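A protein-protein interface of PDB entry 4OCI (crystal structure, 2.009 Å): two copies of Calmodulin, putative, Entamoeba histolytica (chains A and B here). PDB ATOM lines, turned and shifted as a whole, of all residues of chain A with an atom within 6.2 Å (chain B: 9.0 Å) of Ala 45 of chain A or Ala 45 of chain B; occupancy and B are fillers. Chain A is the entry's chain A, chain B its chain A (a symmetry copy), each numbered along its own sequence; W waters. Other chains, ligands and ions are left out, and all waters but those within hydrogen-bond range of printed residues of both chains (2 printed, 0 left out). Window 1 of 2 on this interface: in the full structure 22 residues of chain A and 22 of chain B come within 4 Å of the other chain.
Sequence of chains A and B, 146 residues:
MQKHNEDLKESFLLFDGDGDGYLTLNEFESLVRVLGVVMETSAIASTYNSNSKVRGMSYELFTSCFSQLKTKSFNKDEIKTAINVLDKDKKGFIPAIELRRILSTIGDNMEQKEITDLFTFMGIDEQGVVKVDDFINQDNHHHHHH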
ATOM      1  N   LEU A  25     -28.936  33.274  -0.969  1.00  0.00           N
ATOM      2  CA  LEU A  25     -28.185  32.129  -0.487  1.00  0.00           C
ATOM      3  C   LEU A  25     -26.835  32.551   0.043  1.00  0.00           C
ATOM      4  O   LEU A  25     -26.485  32.171   1.152  1.00  0.00           O
ATOM      5  CB  LEU A  25     -27.965  31.168  -1.684  1.00  0.00           C
ATOM      6  CG  LEU A  25     -27.024  30.008  -1.382  1.00  0.00           C
ATOM      7  CD1 LEU A  25     -27.513  29.121  -0.283  1.00  0.00           C
ATOM      8  CD2 LEU A  25     -26.918  29.264  -2.787  1.00  0.00           C
ATOM      9  N   PHE A  28     -27.264  34.277   3.488  1.00  0.00           N
ATOM     10  CA  PHE A  28     -27.590  33.265   4.499  1.00  0.00           C
ATOM     11  C   PHE A  28     -26.377  32.489   4.964  1.00  0.00           C
ATOM     12  O   PHE A  28     -26.151  32.340   6.173  1.00  0.00           O
ATOM     13  CB  PHE A  28     -28.623  32.314   3.967  1.00  0.00           C
ATOM     14  CG  PHE A  28     -28.976  31.175   4.914  1.00  0.00           C
ATOM     15  CD1 PHE A  28     -29.586  31.430   6.118  1.00  0.00           C
ATOM     16  CD2 PHE A  28     -28.711  29.839   4.579  1.00  0.00           C
ATOM     17  CE1 PHE A  28     -29.968  30.359   7.006  1.00  0.00           C
ATOM     18  CE2 PHE A  28     -29.076  28.799   5.467  1.00  0.00           C
ATOM     19  CZ  PHE A  28     -29.682  29.057   6.655  1.00  0.00           C
ATOM     20  N   GLU A  40     -20.595  22.013   6.231  1.00  0.00           N
ATOM     21  CA  GLU A  40     -20.322  22.045   4.819  1.00  0.00           C
ATOM     22  C   GLU A  40     -21.221  23.085   4.209  1.00  0.00           C
ATOM     23  O   GLU A  40     -22.379  23.154   4.561  1.00  0.00           O
ATOM     24  CB  GLU A  40     -20.700  20.733   4.147  1.00  0.00           C
ATOM     25  CG  GLU A  40     -19.911  19.602   4.601  1.00  0.00           C
ATOM     26  CD  GLU A  40     -20.760  18.382   4.828  1.00  0.00           C
ATOM     27  OE1 GLU A  40     -20.239  17.260   4.580  1.00  0.00           O
ATOM     28  OE2 GLU A  40     -21.934  18.519   5.277  1.00  0.00           O
ATOM     29  N   THR A  41     -20.687  23.814   3.242  1.00  0.00           N
ATOM     30  CA  THR A  41     -21.465  24.754   2.451  1.00  0.00           C
ATOM     31  C   THR A  41     -22.692  24.109   1.841  1.00  0.00           C
ATOM     32  O   THR A  41     -23.784  24.728   1.775  1.00  0.00           O
ATOM     33  CB  THR A  41     -20.556  25.348   1.369  1.00  0.00           C
ATOM     34  OG1 THR A  41     -19.600  26.153   2.056  1.00  0.00           O
ATOM     35  CG2 THR A  41     -21.317  26.273   0.370  1.00  0.00           C
ATOM     36  N   SER A  42     -22.560  22.906   1.323  1.00  0.00           N
ATOM     37  CA  SER A  42     -23.700  22.297   0.587  1.00  0.00           C
ATOM     38  C   SER A  42     -24.794  21.944   1.589  1.00  0.00           C
ATOM     39  O   SER A  42     -25.922  21.816   1.208  1.00  0.00           O
ATOM     40  CB  SER A  42     -23.300  21.033  -0.192  1.00  0.00           C
ATOM     41  OG  SER A  42     -22.866  19.962   0.705  1.00  0.00           O
ATOM     42  N   ALA A  43     -24.469  21.733   2.845  1.00  0.00           N
ATOM     43  CA  ALA A  43     -25.501  21.409   3.851  1.00  0.00           C
ATOM     44  C   ALA A  43     -26.282  22.712   4.234  1.00  0.00           C
ATOM     45  O   ALA A  43     -27.525  22.708   4.386  1.00  0.00           O
ATOM     46  CB  ALA A  43     -24.832  20.775   5.177  1.00  0.00           C
ATOM     47  N   ILE A  44     -25.541  23.788   4.394  1.00  0.00           N
ATOM     48  CA  ILE A  44     -26.142  25.149   4.592  1.00  0.00           C
ATOM     49  C   ILE A  44     -27.057  25.480   3.394  1.00  0.00           C
ATOM     50  O   ILE A  44     -28.172  25.929   3.579  1.00  0.00           O
ATOM     51  CB  ILE A  44     -24.993  26.247   4.715  1.00  0.00           C
ATOM     52  CG1 ILE A  44     -24.215  25.941   6.035  1.00  0.00           C
ATOM     53  CG2 ILE A  44     -25.629  27.700   4.830  1.00  0.00           C
ATOM     54  CD1 ILE A  44     -22.970  26.873   6.349  1.00  0.00           C
ATOM     55  N   ALA A  45     -26.592  25.237   2.173  1.00  0.00           N
ATOM     56  CA  ALA A  45     -27.319  25.549   0.941  1.00  0.00           C
ATOM     57  C   ALA A  45     -28.553  24.693   0.804  1.00  0.00           C
ATOM     58  O   ALA A  45     -29.606  25.153   0.346  1.00  0.00           O
ATOM     59  CB  ALA A  45     -26.365  25.406  -0.334  1.00  0.00           C
ATOM     60  N   SER A  46     -28.437  23.444   1.223  1.00  0.00           N
ATOM     61  CA  SER A  46     -29.551  22.544   1.227  1.00  0.00           C
ATOM     62  C   SER A  46     -30.668  23.022   2.189  1.00  0.00           C
ATOM     63  O   SER A  46     -31.821  22.939   1.882  1.00  0.00           O
ATOM     64  CB  SER A  46     -29.039  21.180   1.688  1.00  0.00           C
ATOM     65  OG  SER A  46     -30.083  20.280   1.640  1.00  0.00           O
ATOM     66  N   THR A  47     -30.313  23.488   3.389  1.00  0.00           N
ATOM     67  CA  THR A  47     -31.300  24.070   4.319  1.00  0.00           C
ATOM     68  C   THR A  47     -31.940  25.298   3.687  1.00  0.00           C
ATOM     69  O   THR A  47     -33.143  25.481   3.749  1.00  0.00           O
ATOM     70  CB  THR A  47     -30.577  24.483   5.653  1.00  0.00           C
ATOM     71  OG1 THR A  47     -29.933  23.312   6.183  1.00  0.00           O
ATOM     72  CG2 THR A  47     -31.535  25.121   6.719  1.00  0.00           C
ATOM     73  N   TYR A  48     -31.119  26.141   3.061  1.00  0.00           N
ATOM     74  CA  TYR A  48     -31.679  27.321   2.355  1.00  0.00           C
ATOM     75  C   TYR A  48     -32.704  26.873   1.276  1.00  0.00           C
ATOM     76  O   TYR A  48     -33.798  27.447   1.161  1.00  0.00           O
ATOM     77  CB  TYR A  48     -30.521  28.131   1.739  1.00  0.00           C
ATOM     78  CG  TYR A  48     -31.008  29.403   1.091  1.00  0.00           C
ATOM     79  CD1 TYR A  48     -31.086  30.577   1.809  1.00  0.00           C
ATOM     80  CD2 TYR A  48     -31.477  29.415  -0.273  1.00  0.00           C
ATOM     81  CE1 TYR A  48     -31.572  31.797   1.190  1.00  0.00           C
ATOM     82  CE2 TYR A  48     -31.969  30.596  -0.888  1.00  0.00           C
ATOM     83  CZ  TYR A  48     -31.984  31.787  -0.152  1.00  0.00           C
ATOM     84  OH  TYR A  48     -32.454  32.943  -0.756  1.00  0.00           O
ATOM     85  N   ASN A  49     -32.347  25.873   0.467  1.00  0.00           N
ATOM     86  CA  ASN A  49     -33.190  25.413  -0.621  1.00  0.00           C
ATOM     87  C   ASN A  49     -34.568  24.932  -0.082  1.00  0.00           C
ATOM     88  O   ASN A  49     -35.614  25.198  -0.657  1.00  0.00           O
ATOM     89  CB  ASN A  49     -32.494  24.285  -1.405  1.00  0.00           C
ATOM     90  CG  ASN A  49     -33.331  23.796  -2.524  1.00  0.00           C
ATOM     91  OD1 ASN A  49     -33.867  22.721  -2.431  1.00  0.00           O
ATOM     92  ND2 ASN A  49     -33.548  24.623  -3.550  1.00  0.00           N
ATOM     93  N   SER A  50     -34.563  24.281   1.060  1.00  0.00           N
ATOM     94  CA  SER A  50     -35.806  23.742   1.630  1.00  0.00           C
ATOM     95  C   SER A  50     -36.600  24.809   2.378  1.00  0.00           C
ATOM     96  O   SER A  50     -37.743  24.602   2.724  1.00  0.00           O
ATOM     97  CB  SER A  50     -35.446  22.653   2.620  1.00  0.00           C
ATOM     98  OG  SER A  50     -35.009  21.536   1.856  1.00  0.00           O
ATOM     99  N   THR B  24     -15.474  18.808  -6.200  1.00  0.00           N
ATOM    100  CA  THR B  24     -15.949  19.703  -5.117  1.00  0.00           C
ATOM    101  C   THR B  24     -17.350  20.229  -5.450  1.00  0.00           C
ATOM    102  O   THR B  24     -17.834  20.023  -6.541  1.00  0.00           O
ATOM    103  CB  THR B  24     -15.067  20.884  -4.899  1.00  0.00           C
ATOM    104  OG1 THR B  24     -15.080  21.682  -6.079  1.00  0.00           O
ATOM    105  CG2 THR B  24     -13.621  20.460  -4.558  1.00  0.00           C
ATOM    106  N   LEU B  25     -18.002  20.935  -4.509  1.00  0.00           N
ATOM    107  CA  LEU B  25     -19.295  21.538  -4.776  1.00  0.00           C
ATOM    108  C   LEU B  25     -19.196  22.565  -5.880  1.00  0.00           C
ATOM    109  O   LEU B  25     -19.981  22.509  -6.817  1.00  0.00           O
ATOM    110  CB  LEU B  25     -19.763  22.251  -3.482  1.00  0.00           C
ATOM    111  CG  LEU B  25     -21.018  23.098  -3.659  1.00  0.00           C
ATOM    112  CD1 LEU B  25     -22.209  22.305  -4.093  1.00  0.00           C
ATOM    113  CD2 LEU B  25     -21.199  23.766  -2.224  1.00  0.00           C
ATOM    114  N   ASN B  26     -18.224  23.469  -5.849  1.00  0.00           N
ATOM    115  CA  ASN B  26     -18.146  24.455  -6.969  1.00  0.00           C
ATOM    116  C   ASN B  26     -17.871  23.853  -8.344  1.00  0.00           C
ATOM    117  O   ASN B  26     -18.441  24.320  -9.328  1.00  0.00           O
ATOM    118  CB  ASN B  26     -17.088  25.517  -6.711  1.00  0.00           C
ATOM    119  CG  ASN B  26     -17.587  26.548  -5.753  1.00  0.00           C
ATOM    120  OD1 ASN B  26     -18.821  26.784  -5.628  1.00  0.00           O
ATOM    121  ND2 ASN B  26     -16.659  27.154  -5.023  1.00  0.00           N
ATOM    122  N   PHE B  28     -18.829  20.777  -9.300  1.00  0.00           N
ATOM    123  CA  PHE B  28     -20.115  20.177  -9.674  1.00  0.00           C
ATOM    124  C   PHE B  28     -21.093  21.188 -10.231  1.00  0.00           C
ATOM    125  O   PHE B  28     -21.691  20.965 -11.293  1.00  0.00           O
ATOM    126  CB  PHE B  28     -20.727  19.484  -8.491  1.00  0.00           C
ATOM    127  CG  PHE B  28     -22.106  18.892  -8.752  1.00  0.00           C
ATOM    128  CD1 PHE B  28     -22.266  17.866  -9.651  1.00  0.00           C
ATOM    129  CD2 PHE B  28     -23.241  19.358  -8.073  1.00  0.00           C
ATOM    130  CE1 PHE B  28     -23.559  17.264  -9.877  1.00  0.00           C
ATOM    131  CE2 PHE B  28     -24.505  18.769  -8.316  1.00  0.00           C
ATOM    132  CZ  PHE B  28     -24.658  17.753  -9.204  1.00  0.00           C
ATOM    133  N   GLU B  29     -21.225  22.325  -9.530  1.00  0.00           N
ATOM    134  CA  GLU B  29     -22.162  23.354  -9.974  1.00  0.00           C
ATOM    135  C   GLU B  29     -21.718  23.922 -11.342  1.00  0.00           C
ATOM    136  O   GLU B  29     -22.528  24.115 -12.277  1.00  0.00           O
ATOM    137  CB  GLU B  29     -22.266  24.517  -8.943  1.00  0.00           C
ATOM    138  CG  GLU B  29     -23.359  25.493  -9.429  1.00  0.00           C
ATOM    139  CD  GLU B  29     -23.352  26.919  -8.776  1.00  0.00           C
ATOM    140  OE1 GLU B  29     -22.578  27.171  -7.773  1.00  0.00           O
ATOM    141  OE2 GLU B  29     -24.146  27.775  -9.313  1.00  0.00           O
ATOM    142  N   VAL B  32     -22.332  21.187 -14.224  1.00  0.00           N
ATOM    143  CA  VAL B  32     -23.774  21.027 -14.495  1.00  0.00           C
ATOM    144  C   VAL B  32     -24.280  22.262 -15.240  1.00  0.00           C
ATOM    145  O   VAL B  32     -25.029  22.131 -16.240  1.00  0.00           O
ATOM    146  CB  VAL B  32     -24.497  20.741 -13.123  1.00  0.00           C
ATOM    147  CG1 VAL B  32     -25.716  21.535 -12.926  1.00  0.00           C
ATOM    148  CG2 VAL B  32     -24.610  19.166 -12.835  1.00  0.00           C
ATOM    149  N   ARG B  33     -23.827  23.460 -14.842  1.00  0.00           N
ATOM    150  CA  ARG B  33     -24.193  24.656 -15.619  1.00  0.00           C
ATOM    151  C   ARG B  33     -23.592  24.695 -17.032  1.00  0.00           C
ATOM    152  O   ARG B  33     -24.320  25.057 -17.992  1.00  0.00           O
ATOM    153  CB  ARG B  33     -23.935  25.940 -14.873  1.00  0.00           C
ATOM    154  CG  ARG B  33     -24.933  26.102 -13.693  1.00  0.00           C
ATOM    155  CD  ARG B  33     -24.694  27.460 -13.104  1.00  0.00           C
ATOM    156  NE  ARG B  33     -25.498  27.726 -11.918  1.00  0.00           N
ATOM    157  CZ  ARG B  33     -26.808  27.876 -11.904  1.00  0.00           C
ATOM    158  NH1 ARG B  33     -27.555  27.721 -13.043  1.00  0.00           N
ATOM    159  NH2 ARG B  33     -27.386  28.160 -10.717  1.00  0.00           N
ATOM    160  N   MET B  39     -31.147  26.147 -13.204  1.00  0.00           N
ATOM    161  CA  MET B  39     -31.813  25.997 -11.916  1.00  0.00           C
ATOM    162  C   MET B  39     -31.047  26.695 -10.772  1.00  0.00           C
ATOM    163  O   MET B  39     -29.931  27.108 -10.970  1.00  0.00           O
ATOM    164  CB  MET B  39     -32.028  24.487 -11.605  1.00  0.00           C
ATOM    165  CG  MET B  39     -30.856  23.795 -11.051  1.00  0.00           C
ATOM    166  SD  MET B  39     -31.128  21.847 -10.708  1.00  0.00           S
ATOM    167  CE  MET B  39     -32.896  21.635  -9.869  1.00  0.00           C
ATOM    168  N   GLU B  40     -31.692  26.849  -9.593  1.00  0.00           N
ATOM    169  CA  GLU B  40     -31.163  27.619  -8.498  1.00  0.00           C
ATOM    170  C   GLU B  40     -29.910  26.933  -8.028  1.00  0.00           C
ATOM    171  O   GLU B  40     -29.892  25.724  -7.929  1.00  0.00           O
ATOM    172  CB  GLU B  40     -32.106  27.610  -7.303  1.00  0.00           C
ATOM    173  CG  GLU B  40     -33.378  28.258  -7.566  1.00  0.00           C
ATOM    174  CD  GLU B  40     -34.532  27.477  -7.000  1.00  0.00           C
ATOM    175  OE1 GLU B  40     -35.519  28.133  -6.567  1.00  0.00           O
ATOM    176  OE2 GLU B  40     -34.484  26.213  -7.003  1.00  0.00           O
ATOM    177  N   THR B  41     -28.918  27.729  -7.664  1.00  0.00           N
ATOM    178  CA  THR B  41     -27.699  27.230  -7.048  1.00  0.00           C
ATOM    179  C   THR B  41     -27.985  26.362  -5.840  1.00  0.00           C
ATOM    180  O   THR B  41     -27.307  25.329  -5.609  1.00  0.00           O
ATOM    181  CB  THR B  41     -26.817  28.427  -6.675  1.00  0.00           C
ATOM    182  OG1 THR B  41     -26.391  29.002  -7.908  1.00  0.00           O
ATOM    183  CG2 THR B  41     -25.537  28.020  -5.881  1.00  0.00           C
ATOM    184  N   SER B  42     -28.919  26.763  -5.004  1.00  0.00           N
ATOM    185  CA  SER B  42     -29.132  26.020  -3.733  1.00  0.00           C
ATOM    186  C   SER B  42     -29.748  24.664  -4.059  1.00  0.00           C
ATOM    187  O   SER B  42     -29.645  23.767  -3.272  1.00  0.00           O
ATOM    188  CB  SER B  42     -30.047  26.769  -2.750  1.00  0.00           C
ATOM    189  OG  SER B  42     -31.401  26.922  -3.283  1.00  0.00           O
ATOM    190  N   ALA B  43     -30.428  24.520  -5.173  1.00  0.00           N
ATOM    191  CA  ALA B  43     -31.023  23.218  -5.536  1.00  0.00           C
ATOM    192  C   ALA B  43     -29.899  22.257  -6.055  1.00  0.00           C
ATOM    193  O   ALA B  43     -29.868  21.049  -5.726  1.00  0.00           O
ATOM    194  CB  ALA B  43     -32.146  23.397  -6.682  1.00  0.00           C
ATOM    195  N   ILE B  44     -29.014  22.807  -6.858  1.00  0.00           N
ATOM    196  CA  ILE B  44     -27.781  22.078  -7.306  1.00  0.00           C
ATOM    197  C   ILE B  44     -26.968  21.645  -6.068  1.00  0.00           C
ATOM    198  O   ILE B  44     -26.538  20.510  -5.981  1.00  0.00           O
ATOM    199  CB  ILE B  44     -26.891  23.018  -8.236  1.00  0.00           C
ATOM    200  CG1 ILE B  44     -27.715  23.278  -9.537  1.00  0.00           C
ATOM    201  CG2 ILE B  44     -25.539  22.280  -8.634  1.00  0.00           C
ATOM    202  CD1 ILE B  44     -27.056  24.249 -10.605  1.00  0.00           C
ATOM    203  N   ALA B  45     -26.779  22.542  -5.106  1.00  0.00           N
ATOM    204  CA  ALA B  45     -25.984  22.297  -3.900  1.00  0.00           C
ATOM    205  C   ALA B  45     -26.638  21.266  -3.016  1.00  0.00           C
ATOM    206  O   ALA B  45     -25.968  20.423  -2.407  1.00  0.00           O
ATOM    207  CB  ALA B  45     -25.718  23.660  -3.108  1.00  0.00           C
ATOM    208  N   SER B  46     -27.958  21.311  -2.958  1.00  0.00           N
ATOM    209  CA  SER B  46     -28.714  20.341  -2.222  1.00  0.00           C
ATOM    210  C   SER B  46     -28.544  18.918  -2.810  1.00  0.00           C
ATOM    211  O   SER B  46     -28.425  17.967  -2.094  1.00  0.00           O
ATOM    212  CB  SER B  46     -30.186  20.747  -2.304  1.00  0.00           C
ATOM    213  OG  SER B  46     -30.927  19.862  -1.550  1.00  0.00           O
ATOM    214  N   THR B  47     -28.578  18.773  -4.137  1.00  0.00           N
ATOM    215  CA  THR B  47     -28.308  17.473  -4.783  1.00  0.00           C
ATOM    216  C   THR B  47     -26.891  17.023  -4.458  1.00  0.00           C
ATOM    217  O   THR B  47     -26.657  15.870  -4.137  1.00  0.00           O
ATOM    218  CB  THR B  47     -28.467  17.624  -6.341  1.00  0.00           C
ATOM    219  OG1 THR B  47     -29.794  18.113  -6.600  1.00  0.00           O
ATOM    220  CG2 THR B  47     -28.198  16.299  -7.134  1.00  0.00           C
ATOM    221  N   TYR B  48     -25.939  17.952  -4.535  1.00  0.00           N
ATOM    222  CA  TYR B  48     -24.545  17.606  -4.158  1.00  0.00           C
ATOM    223  C   TYR B  48     -24.490  17.084  -2.695  1.00  0.00           C
ATOM    224  O   TYR B  48     -23.836  16.069  -2.406  1.00  0.00           O
ATOM    225  CB  TYR B  48     -23.651  18.846  -4.354  1.00  0.00           C
ATOM    226  CG  TYR B  48     -22.199  18.540  -4.089  1.00  0.00           C
ATOM    227  CD1 TYR B  48     -21.367  18.119  -5.104  1.00  0.00           C
ATOM    228  CD2 TYR B  48     -21.653  18.604  -2.754  1.00  0.00           C
ATOM    229  CE1 TYR B  48     -19.974  17.806  -4.845  1.00  0.00           C
ATOM    230  CE2 TYR B  48     -20.296  18.288  -2.482  1.00  0.00           C
ATOM    231  CZ  TYR B  48     -19.461  17.917  -3.542  1.00  0.00           C
ATOM    232  OH  TYR B  48     -18.133  17.618  -3.278  1.00  0.00           O
ATOM    233  N   ASN B  49     -25.146  17.785  -1.768  1.00  0.00           N
ATOM    234  CA  ASN B  49     -25.112  17.436  -0.360  1.00  0.00           C
ATOM    235  C   ASN B  49     -25.656  15.995  -0.138  1.00  0.00           C
ATOM    236  O   ASN B  49     -25.123  15.216   0.640  1.00  0.00           O
ATOM    237  CB  ASN B  49     -25.921  18.451   0.469  1.00  0.00           C
ATOM    238  CG  ASN B  49     -25.903  18.121   1.912  1.00  0.00           C
ATOM    239  OD1 ASN B  49     -26.895  17.669   2.423  1.00  0.00           O
ATOM    240  ND2 ASN B  49     -24.744  18.237   2.564  1.00  0.00           N
ATOM    241  N   SER B  50     -26.680  15.629  -0.877  1.00  0.00           N
ATOM    242  CA  SER B  50     -27.299  14.306  -0.710  1.00  0.00           C
ATOM    243  C   SER B  50     -26.527  13.217  -1.449  1.00  0.00           C
ATOM    244  O   SER B  50     -26.764  12.045  -1.250  1.00  0.00           O
ATOM    245  CB  SER B  50     -28.699  14.356  -1.289  1.00  0.00           C
ATOM    246  OG  SER B  50     -29.486  15.123  -0.387  1.00  0.00           O
ATOM    247  N   ASN B  51     -25.632  13.577  -2.339  1.00  0.00           N
ATOM    248  CA  ASN B  51     -25.011  12.543  -3.190  1.00  0.00           C
ATOM    249  C   ASN B  51     -23.507  12.766  -3.271  1.00  0.00           C
ATOM    250  O   ASN B  51     -22.914  12.888  -4.360  1.00  0.00           O
ATOM    251  CB  ASN B  51     -25.636  12.578  -4.585  1.00  0.00           C
ATOM    252  CG  ASN B  51     -27.122  12.253  -4.549  1.00  0.00           C
ATOM    253  OD1 ASN B  51     -27.523  11.093  -4.464  1.00  0.00           O
ATOM    254  ND2 ASN B  51     -27.944  13.279  -4.568  1.00  0.00           N
ATOM    255  N   SER B  52     -22.875  12.950  -2.145  1.00  0.00           N
ATOM    256  CA  SER B  52     -21.438  13.033  -2.221  1.00  0.00           C
ATOM    257  C   SER B  52     -20.945  12.280  -1.006  1.00  0.00           C
ATOM    258  O   SER B  52     -21.606  12.261   0.028  1.00  0.00           O
ATOM    259  CB  SER B  52     -20.965  14.448  -2.206  1.00  0.00           C
ATOM    260  OG  SER B  52     -21.564  15.170  -1.143  1.00  0.00           O
ATOM    261  N   MET B  57     -17.791  14.213  -4.956  1.00  0.00           N
ATOM    262  CA  MET B  57     -18.702  13.518  -5.800  1.00  0.00           C
ATOM    263  C   MET B  57     -17.943  12.681  -6.848  1.00  0.00           C
ATOM    264  O   MET B  57     -17.169  13.225  -7.576  1.00  0.00           O
ATOM    265  CB  MET B  57     -19.641  14.534  -6.475  1.00  0.00           C
ATOM    266  CG  MET B  57     -20.688  13.768  -7.296  1.00  0.00           C
ATOM    267  SD  MET B  57     -21.714  15.042  -8.219  1.00  0.00           S
ATOM    268  CE  MET B  57     -23.126  14.956  -6.794  1.00  0.00           C
ATOM    269  N   LEU B  69     -31.003  15.885 -12.333  1.00  0.00           N
ATOM    270  CA  LEU B  69     -31.058  17.303 -12.638  1.00  0.00           C
ATOM    271  C   LEU B  69     -31.664  17.584 -14.000  1.00  0.00           C
ATOM    272  O   LEU B  69     -32.459  18.514 -14.139  1.00  0.00           O
ATOM    273  CB  LEU B  69     -29.684  17.997 -12.473  1.00  0.00           C
ATOM    274  CG  LEU B  69     -29.168  17.895 -11.039  1.00  0.00           C
ATOM    275  CD1 LEU B  69     -27.818  18.619 -10.800  1.00  0.00           C
ATOM    276  CD2 LEU B  69     -30.230  18.296  -9.999  1.00  0.00           C
ATOM    277  N   HIS B 146     -29.826  32.212  -5.370  1.00  0.00           N
ATOM    278  CA  HIS B 146     -30.812  31.482  -4.575  1.00  0.00           C
ATOM    279  C   HIS B 146     -30.696  29.933  -4.700  1.00  0.00           C
ATOM    280  O   HIS B 146     -31.660  29.314  -4.081  1.00  0.00           O
ATOM    281  CB  HIS B 146     -32.290  31.980  -4.930  1.00  0.00           C
ATOM    282  CG  HIS B 146     -32.474  33.456  -4.688  1.00  0.00           C
ATOM    283  ND1 HIS B 146     -32.039  34.413  -5.587  1.00  0.00           N
ATOM    284  CD2 HIS B 146     -32.930  34.139  -3.610  1.00  0.00           C
ATOM    285  CE1 HIS B 146     -32.243  35.622  -5.069  1.00  0.00           C
ATOM    286  NE2 HIS B 146     -32.790  35.485  -3.878  1.00  0.00           N
HETATM  287  O   HOH W   1     -29.642  17.689   1.083  1.00  0.00           O
HETATM  288  O   HOH W   2     -33.158  20.664  -0.284  1.00  0.00           O
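The side-chain hydroxyl (OG) of Ser 42 of chain A lies within hydrogen-bond range of the side-chain amide nitrogen (ND2) of Asn 49 of chain B (3.2 Å).
OG of Ser 46 of chain B lies within hydrogen-bond range of OG of Ser 46 of chain A, 3.3 Å away.
The side-chain amide nitrogen (ND2) of Asn 49 of chain A is in hydrogen-bond range of the side-chain hydroxyl (OG) of Ser 42 of chain B, at 3.2 Å.
O of Tyr 48 of chain B sits at hydrogen-bond distance from OG of Ser 52 of chain B (2.8 Å).
O of Ala 43 of chain B is in hydrogen-bond range of OG1 of Thr 47 of chain B (3.1 Å).
The backbone carbonyl oxygen (O) of Ala 43 of chain A is in hydrogen-bond range of the side-chain hydroxyl (OG1) of Thr 47 of chain A, 3.1 Å away.
O of Ser 46 of chain B lies within hydrogen-bond range of OG of Ser 50 of chain B.
OG of Ser 42 of chain B is in hydrogen-bond range of O of His 146 of chain B (2.5 Å).
OG1 of Thr 41 of chain B sits at hydrogen-bond distance from OE2 of Glu 29 of chain B, at 2.9 Å.
Glu 40 of chain A touches Asn 49 of chain B, and with the chains exchanged Asn 49 of chain A touches Glu 40 of chain B.
Ser 42 of chain A touches Ala 45 of chain B, and with the chains exchanged Ala 45 of chain A touches Ser 42 of chain B.
Ala 43 of chain A touches Asn 49 of chain B, and with the chains exchanged Asn 49 of chain A touches Ala 43 of chain B.
Ala 45 of chain A touches its own counterpart, Ala 45 of chain B.
Positions printed for both chains: 25, 28, 40, 41, 42, 43, 44, 45, 46, 47, 48, 49 and 50.
Of the 17 pairs that touch across the chains among the printed residues, 16 have their exchanged pair printed and touching as well.
Along chain B the printed residues that touch a printed residue of chain A span positions 25 to 146.
Printed residues of chain A that touch a printed residue of chain B: Leu 25, Glu 40, Thr 41, Ser 42, Ala 43, Ala 45, Ser 46, Tyr 48 and Asn 49.
Leu 25 of chain A touches Thr 41 of chain B.
Ser 42 of chain B touches Leu 25 of chain A.
Glu 40 of chain A touches Asn 49 of chain B (OE2 to ND2, 3.9 Å).
CB of Ser 42 of chain A touches O of Ala 45 of chain B, 3.5 Å away.
CA of Ala 43 of chain A touches ND2 of Asn 49 of chain B, 3.5 Å away.
CB of Ser 42 of chain B touches O of Ala 45 of chain A (3.5 Å).
Ala 45 of chain A touches Ala 45 of chain B.
Tyr 48 of chain A touches Ser 42 of chain B (CD2 to CB, 3.9 Å).
Asn 49 of chain A touches Glu 40 of chain B.
Ala 43 of chain B touches Asn 49 of chain A.
Water W2 lies within hydrogen-bond range of the side-chain hydroxyl (OG) of Ser 46 of chain B (2.7 Å), the side-chain hydroxyl (OG) of Ser 50 of chain A (3.0 Å), the side-chain amide oxygen (OD1) of Asn 49 of chain A (3.1 Å) and the backbone carbonyl oxygen (O) of Ser 46 of chain A (3.4 Å).
Water W1 lies within hydrogen-bond range of OG of Ser 46 of chain A, OG of Ser 50 of chain B, OD1 of Asn 49 of chain B and O of Ser 46 of chain B.
Ala 45 of chain A touches two residues of chain B.
Of the printed residues of chain A, Ala 45 of chain B touches Ser 42 and Ala 45.
Ser 46 of chain A touches just one residue of chain B: Ser 46.
Of the printed residues of chain A, Glu 40 of chain B touches Asn 49.
Of the printed residues of chain A, His 146 of chain B touches Tyr 48.
Of the printed residues of chain B, Asn 49 of chain A touches Glu 40 (3.9 Å), Ser 42 (3.2 Å) and Ala 43 (3.5 Å).
Printed residues of chain A within 4 Å of Leu 25 of chain B: Thr 41 and Ser 42.
Met 57 of chain B touches none of the printed residues of chain A.
Ser 50 of chain B touches none of the printed residues of chain A.
The nearest printed residue of chain A that does not touch Leu 25 of chain B is Ala 45 of chain A (5.7 Å).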
